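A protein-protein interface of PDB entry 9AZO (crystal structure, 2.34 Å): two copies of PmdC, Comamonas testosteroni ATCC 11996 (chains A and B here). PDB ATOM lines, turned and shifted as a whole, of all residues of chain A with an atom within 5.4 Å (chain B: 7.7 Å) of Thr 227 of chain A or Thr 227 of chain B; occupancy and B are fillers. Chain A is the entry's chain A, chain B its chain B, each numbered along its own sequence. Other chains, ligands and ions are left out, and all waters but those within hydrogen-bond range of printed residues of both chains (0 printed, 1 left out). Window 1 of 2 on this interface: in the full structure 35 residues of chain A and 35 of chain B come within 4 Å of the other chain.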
ATOM      1  N   GLN A 148     -30.310  14.179  13.332  1.00  0.00           N
ATOM      2  CA  GLN A 148     -30.015  13.574  14.628  1.00  0.00           C
ATOM      3  C   GLN A 148     -31.291  13.043  15.284  1.00  0.00           C
ATOM      4  O   GLN A 148     -32.305  13.740  15.319  1.00  0.00           O
ATOM      5  CB  GLN A 148     -29.315  14.593  15.525  1.00  0.00           C
ATOM      6  CG  GLN A 148     -29.017  14.126  16.926  1.00  0.00           C
ATOM      7  CD  GLN A 148     -28.129  15.134  17.655  1.00  0.00           C
ATOM      8  OE1 GLN A 148     -27.511  14.793  18.648  1.00  0.00           O
ATOM      9  NE2 GLN A 148     -28.060  16.376  17.153  1.00  0.00           N
ATOM     10  N   MET A 149     -31.212  11.863  15.889  1.00  0.00           N
ATOM     11  CA  MET A 149     -32.251  11.356  16.794  1.00  0.00           C
ATOM     12  C   MET A 149     -31.756  11.343  18.231  1.00  0.00           C
ATOM     13  O   MET A 149     -30.743  10.694  18.514  1.00  0.00           O
ATOM     14  CB  MET A 149     -32.702   9.933  16.456  1.00  0.00           C
ATOM     15  CG  MET A 149     -33.750   9.798  15.381  1.00  0.00           C
ATOM     16  SD  MET A 149     -33.960   8.043  15.010  1.00  0.00           S
ATOM     17  CE  MET A 149     -34.566   7.410  16.590  1.00  0.00           C
ATOM     18  N   ASP A 150     -32.453  12.059  19.130  1.00  0.00           N
ATOM     19  CA  ASP A 150     -32.109  12.045  20.549  1.00  0.00           C
ATOM     20  C   ASP A 150     -33.195  11.289  21.336  1.00  0.00           C
ATOM     21  O   ASP A 150     -34.361  11.712  21.349  1.00  0.00           O
ATOM     22  CB  ASP A 150     -31.959  13.462  21.101  1.00  0.00           C
ATOM     23  CG  ASP A 150     -31.694  13.467  22.598  1.00  0.00           C
ATOM     24  OD1 ASP A 150     -30.901  12.605  23.037  1.00  0.00           O
ATOM     25  OD2 ASP A 150     -32.312  14.246  23.347  1.00  0.00           O
ATOM     26  N   VAL A 151     -32.816  10.189  22.000  1.00  0.00           N
ATOM     27  CA  VAL A 151     -33.753   9.231  22.574  1.00  0.00           C
ATOM     28  C   VAL A 151     -33.456   8.955  24.047  1.00  0.00           C
ATOM     29  O   VAL A 151     -32.299   8.723  24.428  1.00  0.00           O
ATOM     30  CB  VAL A 151     -33.753   7.917  21.776  1.00  0.00           C
ATOM     31  CG1 VAL A 151     -34.862   7.037  22.235  1.00  0.00           C
ATOM     32  CG2 VAL A 151     -33.907   8.207  20.290  1.00  0.00           C
ATOM     33  N   MET A 214     -26.890   3.201  30.929  1.00  0.00           N
ATOM     34  CA  MET A 214     -26.142   2.937  29.714  1.00  0.00           C
ATOM     35  C   MET A 214     -26.314   4.115  28.759  1.00  0.00           C
ATOM     36  O   MET A 214     -27.377   4.742  28.723  1.00  0.00           O
ATOM     37  CB  MET A 214     -26.549   1.584  29.118  1.00  0.00           C
ATOM     38  CG  MET A 214     -25.711   1.167  27.919  1.00  0.00           C
ATOM     39  SD  MET A 214     -26.174  -0.487  27.437  1.00  0.00           S
ATOM     40  CE  MET A 214     -27.713  -0.179  26.620  1.00  0.00           C
ATOM     41  N   SER A 215     -25.249   4.419  28.006  1.00  0.00           N
ATOM     42  CA  SER A 215     -25.247   5.445  26.967  1.00  0.00           C
ATOM     43  C   SER A 215     -24.743   4.928  25.623  1.00  0.00           C
ATOM     44  O   SER A 215     -23.676   4.313  25.552  1.00  0.00           O
ATOM     45  CB  SER A 215     -24.376   6.617  27.413  1.00  0.00           C
ATOM     46  OG  SER A 215     -24.399   7.662  26.459  1.00  0.00           O
ATOM     47  N   ILE A 216     -25.519   5.150  24.564  1.00  0.00           N
ATOM     48  CA  ILE A 216     -25.196   4.665  23.227  1.00  0.00           C
ATOM     49  C   ILE A 216     -25.191   5.820  22.240  1.00  0.00           C
ATOM     50  O   ILE A 216     -26.124   6.635  22.214  1.00  0.00           O
ATOM     51  CB  ILE A 216     -26.214   3.600  22.785  1.00  0.00           C
ATOM     52  CG1 ILE A 216     -26.101   2.389  23.714  1.00  0.00           C
ATOM     53  CG2 ILE A 216     -26.102   3.307  21.305  1.00  0.00           C
ATOM     54  CD1 ILE A 216     -27.127   1.364  23.482  1.00  0.00           C
ATOM     55  N   GLN A 217     -24.185   5.837  21.365  1.00  0.00           N
ATOM     56  CA  GLN A 217     -24.088   6.763  20.241  1.00  0.00           C
ATOM     57  C   GLN A 217     -23.935   6.029  18.910  1.00  0.00           C
ATOM     58  O   GLN A 217     -23.170   5.056  18.815  1.00  0.00           O
ATOM     59  CB  GLN A 217     -23.017   7.817  20.545  1.00  0.00           C
ATOM     60  CG  GLN A 217     -21.600   7.370  20.769  1.00  0.00           C
ATOM     61  CD  GLN A 217     -20.659   8.584  20.893  1.00  0.00           C
ATOM     62  OE1 GLN A 217     -19.457   8.459  20.711  1.00  0.00           O
ATOM     63  NE2 GLN A 217     -21.221   9.756  21.254  1.00  0.00           N
ATOM     64  N   LEU A 218     -24.744   6.423  17.917  1.00  0.00           N
ATOM     65  CA  LEU A 218     -24.721   5.817  16.589  1.00  0.00           C
ATOM     66  C   LEU A 218     -24.442   6.855  15.515  1.00  0.00           C
ATOM     67  O   LEU A 218     -24.819   8.012  15.648  1.00  0.00           O
ATOM     68  CB  LEU A 218     -26.054   5.198  16.259  1.00  0.00           C
ATOM     69  CG  LEU A 218     -26.647   4.340  17.363  1.00  0.00           C
ATOM     70  CD1 LEU A 218     -28.091   3.998  16.967  1.00  0.00           C
ATOM     71  CD2 LEU A 218     -25.757   3.097  17.670  1.00  0.00           C
ATOM     72  N   ILE A 225     -26.762  11.052  12.978  1.00  0.00           N
ATOM     73  CA  ILE A 225     -26.293  10.539  14.268  1.00  0.00           C
ATOM     74  C   ILE A 225     -27.515  10.328  15.163  1.00  0.00           C
ATOM     75  O   ILE A 225     -28.561  10.950  14.995  1.00  0.00           O
ATOM     76  CB  ILE A 225     -25.250  11.405  15.007  1.00  0.00           C
ATOM     77  CG1 ILE A 225     -25.779  12.795  15.340  1.00  0.00           C
ATOM     78  CG2 ILE A 225     -23.979  11.548  14.185  1.00  0.00           C
ATOM     79  CD1 ILE A 225     -24.843  13.525  16.307  1.00  0.00           C
ATOM     80  N   CYS A 226     -27.360   9.438  16.123  1.00  0.00           N
ATOM     81  CA  CYS A 226     -28.332   9.195  17.173  1.00  0.00           C
ATOM     82  C   CYS A 226     -27.646   9.190  18.535  1.00  0.00           C
ATOM     83  O   CYS A 226     -26.624   8.516  18.716  1.00  0.00           O
ATOM     84  CB  CYS A 226     -29.069   7.877  16.902  1.00  0.00           C
ATOM     85  SG  CYS A 226     -30.316   7.430  18.126  1.00  0.00           S
ATOM     86  N   THR A 227     -28.271   9.855  19.515  1.00  0.00           N
ATOM     87  CA  THR A 227     -27.898   9.763  20.927  1.00  0.00           C
ATOM     88  C   THR A 227     -28.978   9.049  21.734  1.00  0.00           C
ATOM     89  O   THR A 227     -30.164   9.370  21.610  1.00  0.00           O
ATOM     90  CB  THR A 227     -27.749  11.178  21.480  1.00  0.00           C
ATOM     91  OG1 THR A 227     -26.795  11.909  20.704  1.00  0.00           O
ATOM     92  CG2 THR A 227     -27.278  11.121  22.894  1.00  0.00           C
ATOM     93  N   LEU A 228     -28.578   8.042  22.510  1.00  0.00           N
ATOM     94  CA  LEU A 228     -29.502   7.239  23.305  1.00  0.00           C
ATOM     95  C   LEU A 228     -29.062   7.147  24.762  1.00  0.00           C
ATOM     96  O   LEU A 228     -27.982   6.603  25.047  1.00  0.00           O
ATOM     97  CB  LEU A 228     -29.606   5.833  22.712  1.00  0.00           C
ATOM     98  CG  LEU A 228     -30.324   4.792  23.536  1.00  0.00           C
ATOM     99  CD1 LEU A 228     -31.787   5.270  23.636  1.00  0.00           C
ATOM    100  CD2 LEU A 228     -30.205   3.399  22.940  1.00  0.00           C
ATOM    101  N   SER A 229     -29.902   7.633  25.677  1.00  0.00           N
ATOM    102  CA  SER A 229     -29.732   7.422  27.119  1.00  0.00           C
ATOM    103  C   SER A 229     -30.682   6.346  27.660  1.00  0.00           C
ATOM    104  O   SER A 229     -31.888   6.444  27.429  1.00  0.00           O
ATOM    105  CB  SER A 229     -29.971   8.735  27.871  1.00  0.00           C
ATOM    106  OG  SER A 229     -29.803   8.551  29.265  1.00  0.00           O
ATOM    107  N   GLN B 148     -26.366   9.007  36.388  1.00  0.00           N
ATOM    108  CA  GLN B 148     -26.329   9.477  35.006  1.00  0.00           C
ATOM    109  C   GLN B 148     -26.835  10.916  34.876  1.00  0.00           C
ATOM    110  O   GLN B 148     -27.861  11.288  35.463  1.00  0.00           O
ATOM    111  CB  GLN B 148     -27.115   8.573  34.045  1.00  0.00           C
ATOM    112  CG  GLN B 148     -27.128   9.149  32.611  1.00  0.00           C
ATOM    113  CD  GLN B 148     -27.704   8.197  31.581  1.00  0.00           C
ATOM    114  OE1 GLN B 148     -27.520   8.396  30.369  1.00  0.00           O
ATOM    115  NE2 GLN B 148     -28.395   7.141  32.052  1.00  0.00           N
ATOM    116  N   MET B 149     -26.142  11.698  34.052  1.00  0.00           N
ATOM    117  CA  MET B 149     -26.606  12.995  33.555  1.00  0.00           C
ATOM    118  C   MET B 149     -26.929  12.930  32.067  1.00  0.00           C
ATOM    119  O   MET B 149     -26.076  12.532  31.273  1.00  0.00           O
ATOM    120  CB  MET B 149     -25.599  14.120  33.773  1.00  0.00           C
ATOM    121  CG  MET B 149     -25.609  14.741  35.114  1.00  0.00           C
ATOM    122  SD  MET B 149     -24.245  15.901  35.316  1.00  0.00           S
ATOM    123  CE  MET B 149     -24.671  17.113  34.066  1.00  0.00           C
ATOM    124  N   ASP B 150     -28.169  13.269  31.709  1.00  0.00           N
ATOM    125  CA  ASP B 150     -28.675  13.362  30.338  1.00  0.00           C
ATOM    126  C   ASP B 150     -28.908  14.819  29.936  1.00  0.00           C
ATOM    127  O   ASP B 150     -29.585  15.540  30.665  1.00  0.00           O
ATOM    128  CB  ASP B 150     -29.982  12.579  30.205  1.00  0.00           C
ATOM    129  CG  ASP B 150     -30.624  12.752  28.857  1.00  0.00           C
ATOM    130  OD1 ASP B 150     -29.892  12.763  27.864  1.00  0.00           O
ATOM    131  OD2 ASP B 150     -31.857  12.889  28.779  1.00  0.00           O
ATOM    132  N   VAL B 151     -28.218  15.297  28.891  1.00  0.00           N
ATOM    133  CA  VAL B 151     -28.160  16.718  28.539  1.00  0.00           C
ATOM    134  C   VAL B 151     -28.505  16.974  27.060  1.00  0.00           C
ATOM    135  O   VAL B 151     -28.058  16.248  26.169  1.00  0.00           O
ATOM    136  CB  VAL B 151     -26.782  17.326  28.858  1.00  0.00           C
ATOM    137  CG1 VAL B 151     -26.832  18.834  28.704  1.00  0.00           C
ATOM    138  CG2 VAL B 151     -26.292  16.890  30.260  1.00  0.00           C
ATOM    139  N   GLN B 152     -29.306  18.016  26.803  1.00  0.00           N
ATOM    140  CA  GLN B 152     -29.635  18.495  25.455  1.00  0.00           C
ATOM    141  C   GLN B 152     -29.235  19.964  25.384  1.00  0.00           C
ATOM    142  O   GLN B 152     -29.599  20.740  26.271  1.00  0.00           O
ATOM    143  CB  GLN B 152     -31.128  18.341  25.128  1.00  0.00           C
ATOM    144  CG  GLN B 152     -31.635  16.890  25.005  1.00  0.00           C
ATOM    145  CD  GLN B 152     -31.873  16.234  26.346  1.00  0.00           C
ATOM    146  OE1 GLN B 152     -32.376  16.857  27.267  1.00  0.00           O
ATOM    147  NE2 GLN B 152     -31.529  14.963  26.453  1.00  0.00           N
ATOM    148  N   TYR B 154     -29.477  22.657  22.480  1.00  0.00           N
ATOM    149  CA  TYR B 154     -30.170  22.831  21.209  1.00  0.00           C
ATOM    150  C   TYR B 154     -30.368  24.287  20.823  1.00  0.00           C
ATOM    151  O   TYR B 154     -30.664  25.120  21.681  1.00  0.00           O
ATOM    152  CB  TYR B 154     -31.536  22.151  21.222  1.00  0.00           C
ATOM    153  CG  TYR B 154     -31.497  20.663  21.310  1.00  0.00           C
ATOM    154  CD1 TYR B 154     -30.394  19.949  20.853  1.00  0.00           C
ATOM    155  CD2 TYR B 154     -32.572  19.961  21.827  1.00  0.00           C
ATOM    156  CE1 TYR B 154     -30.360  18.564  20.930  1.00  0.00           C
ATOM    157  CE2 TYR B 154     -32.556  18.594  21.911  1.00  0.00           C
ATOM    158  CZ  TYR B 154     -31.454  17.888  21.461  1.00  0.00           C
ATOM    159  OH  TYR B 154     -31.449  16.500  21.562  1.00  0.00           O
ATOM    160  N   THR B 182     -21.052  21.224  29.809  1.00  0.00           N
ATOM    161  CA  THR B 182     -21.417  19.932  30.350  1.00  0.00           C
ATOM    162  C   THR B 182     -20.181  19.104  30.684  1.00  0.00           C
ATOM    163  O   THR B 182     -20.149  18.428  31.713  1.00  0.00           O
ATOM    164  CB  THR B 182     -22.368  19.205  29.396  1.00  0.00           C
ATOM    165  OG1 THR B 182     -23.559  19.996  29.202  1.00  0.00           O
ATOM    166  CG2 THR B 182     -22.702  17.795  29.903  1.00  0.00           C
ATOM    167  N   PHE B 186     -20.216  18.009  34.473  1.00  0.00           N
ATOM    168  CA  PHE B 186     -20.284  16.593  34.834  1.00  0.00           C
ATOM    169  C   PHE B 186     -19.218  16.172  35.845  1.00  0.00           C
ATOM    170  O   PHE B 186     -19.523  15.481  36.821  1.00  0.00           O
ATOM    171  CB  PHE B 186     -20.172  15.739  33.576  1.00  0.00           C
ATOM    172  CG  PHE B 186     -20.170  14.242  33.847  1.00  0.00           C
ATOM    173  CD1 PHE B 186     -21.300  13.606  34.384  1.00  0.00           C
ATOM    174  CD2 PHE B 186     -19.040  13.481  33.571  1.00  0.00           C
ATOM    175  CE1 PHE B 186     -21.307  12.228  34.624  1.00  0.00           C
ATOM    176  CE2 PHE B 186     -19.034  12.093  33.816  1.00  0.00           C
ATOM    177  CZ  PHE B 186     -20.155  11.463  34.332  1.00  0.00           C
ATOM    178  N   VAL B 200     -19.334  11.414  18.247  1.00  0.00           N
ATOM    179  CA  VAL B 200     -19.554  11.350  16.802  1.00  0.00           C
ATOM    180  C   VAL B 200     -20.270  12.638  16.401  1.00  0.00           C
ATOM    181  O   VAL B 200     -20.899  13.289  17.238  1.00  0.00           O
ATOM    182  CB  VAL B 200     -20.387  10.120  16.377  1.00  0.00           C
ATOM    183  CG1 VAL B 200     -19.658   8.861  16.668  1.00  0.00           C
ATOM    184  CG2 VAL B 200     -21.771  10.124  17.072  1.00  0.00           C
ATOM    185  N   MET B 214     -23.887  16.870  17.165  1.00  0.00           N
ATOM    186  CA  MET B 214     -22.796  16.181  17.830  1.00  0.00           C
ATOM    187  C   MET B 214     -23.370  15.348  18.970  1.00  0.00           C
ATOM    188  O   MET B 214     -24.338  15.762  19.625  1.00  0.00           O
ATOM    189  CB  MET B 214     -21.763  17.186  18.326  1.00  0.00           C
ATOM    190  CG  MET B 214     -20.484  16.595  18.918  1.00  0.00           C
ATOM    191  SD  MET B 214     -19.404  18.014  19.258  1.00  0.00           S
ATOM    192  CE  MET B 214     -19.016  18.506  17.567  1.00  0.00           C
ATOM    193  N   SER B 215     -22.773  14.187  19.217  1.00  0.00           N
ATOM    194  CA  SER B 215     -23.156  13.359  20.353  1.00  0.00           C
ATOM    195  C   SER B 215     -21.931  13.023  21.183  1.00  0.00           C
ATOM    196  O   SER B 215     -20.897  12.615  20.635  1.00  0.00           O
ATOM    197  CB  SER B 215     -23.841  12.065  19.892  1.00  0.00           C
ATOM    198  OG  SER B 215     -24.279  11.279  21.006  1.00  0.00           O
ATOM    199  N   ILE B 216     -22.009  13.285  22.489  1.00  0.00           N
ATOM    200  CA  ILE B 216     -20.877  13.059  23.377  1.00  0.00           C
ATOM    201  C   ILE B 216     -21.327  12.153  24.511  1.00  0.00           C
ATOM    202  O   ILE B 216     -22.390  12.354  25.106  1.00  0.00           O
ATOM    203  CB  ILE B 216     -20.306  14.405  23.868  1.00  0.00           C
ATOM    204  CG1 ILE B 216     -19.763  15.149  22.642  1.00  0.00           C
ATOM    205  CG2 ILE B 216     -19.243  14.222  24.933  1.00  0.00           C
ATOM    206  CD1 ILE B 216     -19.312  16.557  22.902  1.00  0.00           C
ATOM    207  N   GLN B 217     -20.492  11.181  24.844  1.00  0.00           N
ATOM    208  CA  GLN B 217     -20.689  10.309  25.990  1.00  0.00           C
ATOM    209  C   GLN B 217     -19.475  10.347  26.909  1.00  0.00           C
ATOM    210  O   GLN B 217     -18.344  10.271  26.435  1.00  0.00           O
ATOM    211  CB  GLN B 217     -21.062   8.950  25.433  1.00  0.00           C
ATOM    212  CG  GLN B 217     -20.000   8.170  24.771  1.00  0.00           C
ATOM    213  CD  GLN B 217     -20.550   6.815  24.420  1.00  0.00           C
ATOM    214  OE1 GLN B 217     -21.785   6.649  24.382  1.00  0.00           O
ATOM    215  NE2 GLN B 217     -19.677   5.812  24.289  1.00  0.00           N
ATOM    216  N   LEU B 218     -19.703  10.535  28.201  1.00  0.00           N
ATOM    217  CA  LEU B 218     -18.650  10.604  29.206  1.00  0.00           C
ATOM    218  C   LEU B 218     -18.852   9.548  30.284  1.00  0.00           C
ATOM    219  O   LEU B 218     -19.979   9.190  30.620  1.00  0.00           O
ATOM    220  CB  LEU B 218     -18.653  11.994  29.880  1.00  0.00           C
ATOM    221  CG  LEU B 218     -18.732  13.196  28.947  1.00  0.00           C
ATOM    222  CD1 LEU B 218     -18.970  14.483  29.744  1.00  0.00           C
ATOM    223  CD2 LEU B 218     -17.457  13.279  28.046  1.00  0.00           C
ATOM    224  N   LYS B 219     -17.745   9.064  30.841  1.00  0.00           N
ATOM    225  CA  LYS B 219     -17.755   8.206  32.020  1.00  0.00           C
ATOM    226  C   LYS B 219     -16.747   8.744  33.021  1.00  0.00           C
ATOM    227  O   LYS B 219     -15.596   9.021  32.660  1.00  0.00           O
ATOM    228  CB  LYS B 219     -17.437   6.740  31.667  1.00  0.00           C
ATOM    229  CG  LYS B 219     -17.496   5.708  32.848  1.00  0.00           C
ATOM    230  CD  LYS B 219     -17.235   4.300  32.272  1.00  0.00           C
ATOM    231  CE  LYS B 219     -17.249   3.167  33.287  1.00  0.00           C
ATOM    232  NZ  LYS B 219     -18.561   2.993  33.913  1.00  0.00           N
ATOM    233  N   ILE B 225     -22.115   8.105  34.523  1.00  0.00           N
ATOM    234  CA  ILE B 225     -22.040   8.372  33.081  1.00  0.00           C
ATOM    235  C   ILE B 225     -22.813   9.656  32.734  1.00  0.00           C
ATOM    236  O   ILE B 225     -23.728  10.091  33.448  1.00  0.00           O
ATOM    237  CB  ILE B 225     -22.486   7.178  32.202  1.00  0.00           C
ATOM    238  CG1 ILE B 225     -23.935   6.770  32.475  1.00  0.00           C
ATOM    239  CG2 ILE B 225     -21.531   6.014  32.398  1.00  0.00           C
ATOM    240  CD1 ILE B 225     -24.486   5.774  31.427  1.00  0.00           C
ATOM    241  N   CYS B 226     -22.428  10.258  31.599  1.00  0.00           N
ATOM    242  CA  CYS B 226     -23.129  11.400  31.024  1.00  0.00           C
ATOM    243  C   CYS B 226     -23.417  11.158  29.547  1.00  0.00           C
ATOM    244  O   CYS B 226     -22.524  10.763  28.792  1.00  0.00           O
ATOM    245  CB  CYS B 226     -22.272  12.659  31.199  1.00  0.00           C
ATOM    246  SG  CYS B 226     -23.037  14.152  30.538  1.00  0.00           S
ATOM    247  N   THR B 227     -24.652  11.475  29.128  1.00  0.00           N
ATOM    248  CA  THR B 227     -25.047  11.533  27.721  1.00  0.00           C
ATOM    249  C   THR B 227     -25.355  12.976  27.317  1.00  0.00           C
ATOM    250  O   THR B 227     -26.134  13.646  27.990  1.00  0.00           O
ATOM    251  CB  THR B 227     -26.315  10.675  27.581  1.00  0.00           C
ATOM    252  OG1 THR B 227     -26.060   9.353  28.065  1.00  0.00           O
ATOM    253  CG2 THR B 227     -26.715  10.545  26.145  1.00  0.00           C
ATOM    254  N   LEU B 228     -24.742  13.458  26.229  1.00  0.00           N
ATOM    255  CA  LEU B 228     -24.904  14.830  25.748  1.00  0.00           C
ATOM    256  C   LEU B 228     -25.262  14.868  24.265  1.00  0.00           C
ATOM    257  O   LEU B 228     -24.533  14.311  23.442  1.00  0.00           O
ATOM    258  CB  LEU B 228     -23.632  15.627  26.032  1.00  0.00           C
ATOM    259  CG  LEU B 228     -23.471  16.993  25.400  1.00  0.00           C
ATOM    260  CD1 LEU B 228     -24.580  17.904  25.964  1.00  0.00           C
ATOM    261  CD2 LEU B 228     -22.090  17.526  25.732  1.00  0.00           C
ATOM    262  N   SER B 229     -26.420  15.431  23.931  1.00  0.00           N
ATOM    263  CA  SER B 229     -26.810  15.730  22.557  1.00  0.00           C
ATOM    264  C   SER B 229     -26.652  17.227  22.259  1.00  0.00           C
ATOM    265  O   SER B 229     -27.115  18.052  23.052  1.00  0.00           O
ATOM    266  CB  SER B 229     -28.232  15.210  22.337  1.00  0.00           C
ATOM    267  OG  SER B 229     -28.693  15.436  21.026  1.00  0.00           O
ATOM    268  N   LEU B 230     -25.919  17.590  21.181  1.00  0.00           N
ATOM    269  CA  LEU B 230     -25.805  18.990  20.748  1.00  0.00           C
ATOM    270  C   LEU B 230     -26.333  19.199  19.329  1.00  0.00           C
ATOM    271  O   LEU B 230     -26.127  18.356  18.453  1.00  0.00           O
ATOM    272  CB  LEU B 230     -24.368  19.518  20.836  1.00  0.00           C
ATOM    273  CG  LEU B 230     -23.642  19.226  22.149  1.00  0.00           C
ATOM    274  CD1 LEU B 230     -22.626  18.064  22.003  1.00  0.00           C
ATOM    275  CD2 LEU B 230     -23.064  20.488  22.788  1.00  0.00           C
ATOM    276  N   PHE B 241     -31.119  21.783  28.658  1.00  0.00           N
ATOM    277  CA  PHE B 241     -31.959  21.044  29.592  1.00  0.00           C
ATOM    278  C   PHE B 241     -31.089  19.941  30.199  1.00  0.00           C
ATOM    279  O   PHE B 241     -30.418  19.207  29.462  1.00  0.00           O
ATOM    280  CB  PHE B 241     -33.223  20.492  28.911  1.00  0.00           C
ATOM    281  CG  PHE B 241     -34.018  21.530  28.116  1.00  0.00           C
ATOM    282  CD1 PHE B 241     -33.552  22.072  26.935  1.00  0.00           C
ATOM    283  CD2 PHE B 241     -35.255  21.956  28.588  1.00  0.00           C
ATOM    284  CE1 PHE B 241     -34.295  23.010  26.243  1.00  0.00           C
ATOM    285  CE2 PHE B 241     -36.010  22.905  27.907  1.00  0.00           C
ATOM    286  CZ  PHE B 241     -35.540  23.427  26.738  1.00  0.00           C
ATOM    287  N   ARG B 243     -30.816  16.639  32.930  1.00  0.00           N
ATOM    288  CA  ARG B 243     -31.383  15.630  33.812  1.00  0.00           C
ATOM    289  C   ARG B 243     -30.319  14.928  34.657  1.00  0.00           C
ATOM    290  O   ARG B 243     -29.373  14.377  34.106  1.00  0.00           O
ATOM    291  CB  ARG B 243     -32.215  14.634  33.028  1.00  0.00           C
ATOM    292  CG  ARG B 243     -32.708  13.590  33.940  1.00  0.00           C
ATOM    293  CD  ARG B 243     -33.380  12.487  33.235  1.00  0.00           C
ATOM    294  NE  ARG B 243     -34.480  13.135  32.524  1.00  0.00           N
ATOM    295  CZ  ARG B 243     -35.770  12.940  32.768  1.00  0.00           C
ATOM    296  NH1 ARG B 243     -36.184  12.093  33.692  1.00  0.00           N
ATOM    297  NH2 ARG B 243     -36.667  13.587  32.036  1.00  0.00           N
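Met 214 of chain A touches Ile 225 of chain B, and with the chains exchanged Ile 225 of chain A touches Met 214 of chain B. Ser 215 of chain A touches Ile 225 of chain B, and with the chains exchanged Ile 225 of chain A touches Ser 215 of chain B. Positions printed for both chains: 148, 149, 150, 151, 214, 215, 216, 217, 218, 225, 226, 227, 228 and 229. Of the 23 pairs that touch across the chains among the printed residues, 14 have their exchanged pair printed and touching as well.
The side-chain amide oxygen (OE1) of Gln 148 of chain A lies close to the backbone carbonyl oxygen (O) of Met 214 of chain B (3.5 Å). The side-chain amide oxygen of Gln 148 of chain A lies within hydrogen-bond range of the side-chain hydroxyl of Ser 229 of chain B, at 2.7 Å. O of Leu 230 of chain B sits at hydrogen-bond distance from NE2 of Gln 148 of chain A, 3.1 Å away. The side-chain amide nitrogen of Gln 152 of chain B lies close to the side-chain carboxylate of Asp 150 of chain A, 3.3 Å away. The side-chain carboxylate of Asp 150 of chain A lies within hydrogen-bond range of the side-chain hydroxyl of Tyr 154 of chain B, at 3.0 Å. O of Ser 215 of chain A lies close to OE1 of Gln 217 of chain B. OG of Ser 215 of chain A lies within hydrogen-bond range of OG1 of Thr 227 of chain B (2.9 Å). The backbone carbonyl oxygen (O) of Ser 215 of chain B sits at hydrogen-bond distance from the side-chain amide nitrogen (NE2) of Gln 217 of chain A (2.9 Å). OG1 of Thr 227 of chain A sits at hydrogen-bond distance from OG of Ser 215 of chain B (2.6 Å). The side-chain amide oxygen of Gln 148 of chain B is in hydrogen-bond range of the side-chain hydroxyl of Ser 229 of chain A, at 2.5 Å.
Of chain B, only Ser 215, Thr 227 and Ser 229 come within 4 Å of Thr 227 of chain A. Thr 227 of chain B touches just these residues of chain A: Ser 215, Thr 227 and Ser 229. Of the printed residues of chain A, Met 214 of chain B touches Gln 148 and Ile 225. Printed residues of chain B within 4 Å of Gln 148 of chain A: Met 214 (3.5 Å), Ser 229 (2.7 Å) and Leu 230 (3.1 Å). Of the printed residues of chain A, Tyr 154 of chain B touches Asp 150 (3.0 Å). Of the printed residues of chain A, Leu 230 of chain B touches Gln 148. Printed residues of chain A within 4 Å of Ser 229 of chain B: Gln 148 (2.7 Å), Asp 150 (3.8 Å) and Thr 227 (3.95 Å). The nearest residue of chain B that does not touch Thr 227 of chain A is Leu 228 of chain B (4.2 Å). The nearest printed residue of chain B that does not touch Ile 225 of chain A is Leu 230 of chain B (5.4 Å).
Ser 215 of chain A touches Ile 225 of chain B. OE1 of Gln 217 of chain B touches CG of Gln 217 of chain A, at 3.7 Å. CG2 of Val 200 of chain B touches CG2 of Ile 225 of chain A, at 3.9 Å. Met 214 of chain B touches Ile 225 of chain A. Ile 225 of chain A touches Ser 215 of chain B. Thr 227 of chain A touches Thr 227 of chain B (CG2 to CG2, 3.3 Å). Thr 227 of chain A touches Ser 229 of chain B. Ser 229 of chain A touches Thr 227 of chain B.
Of the 23 printed residues of chain B, 12 touch a printed residue of chain A. Hydrophobic or aromatic side chains of chain B that line the printed part of chain A: Tyr 154, Val 200 and Ile 225. Of the 14 printed residues of chain A, 9 touch a printed residue of chain B. Along chain A the printed residues that touch a printed residue of chain B span positions 148 to 229. Among the printed residues, 23 pairs touch across the chains.
The backbone carbonyl oxygen (O) of Val 151 of chain A sits at hydrogen-bond distance from the backbone NH (N) of Ser 229 of chain A (2.9 Å). OE1 of Gln 148 of chain B is in hydrogen-bond range of OG1 of Thr 227 of chain B. The backbone NH of Thr 227 of chain B lies within hydrogen-bond range of the backbone carbonyl oxygen of Met 149 of chain B, 2.8 Å away. NE2 of Gln 152 of chain B lies within hydrogen-bond range of OD1 of Asp 150 of chain B, 3.1 Å away.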
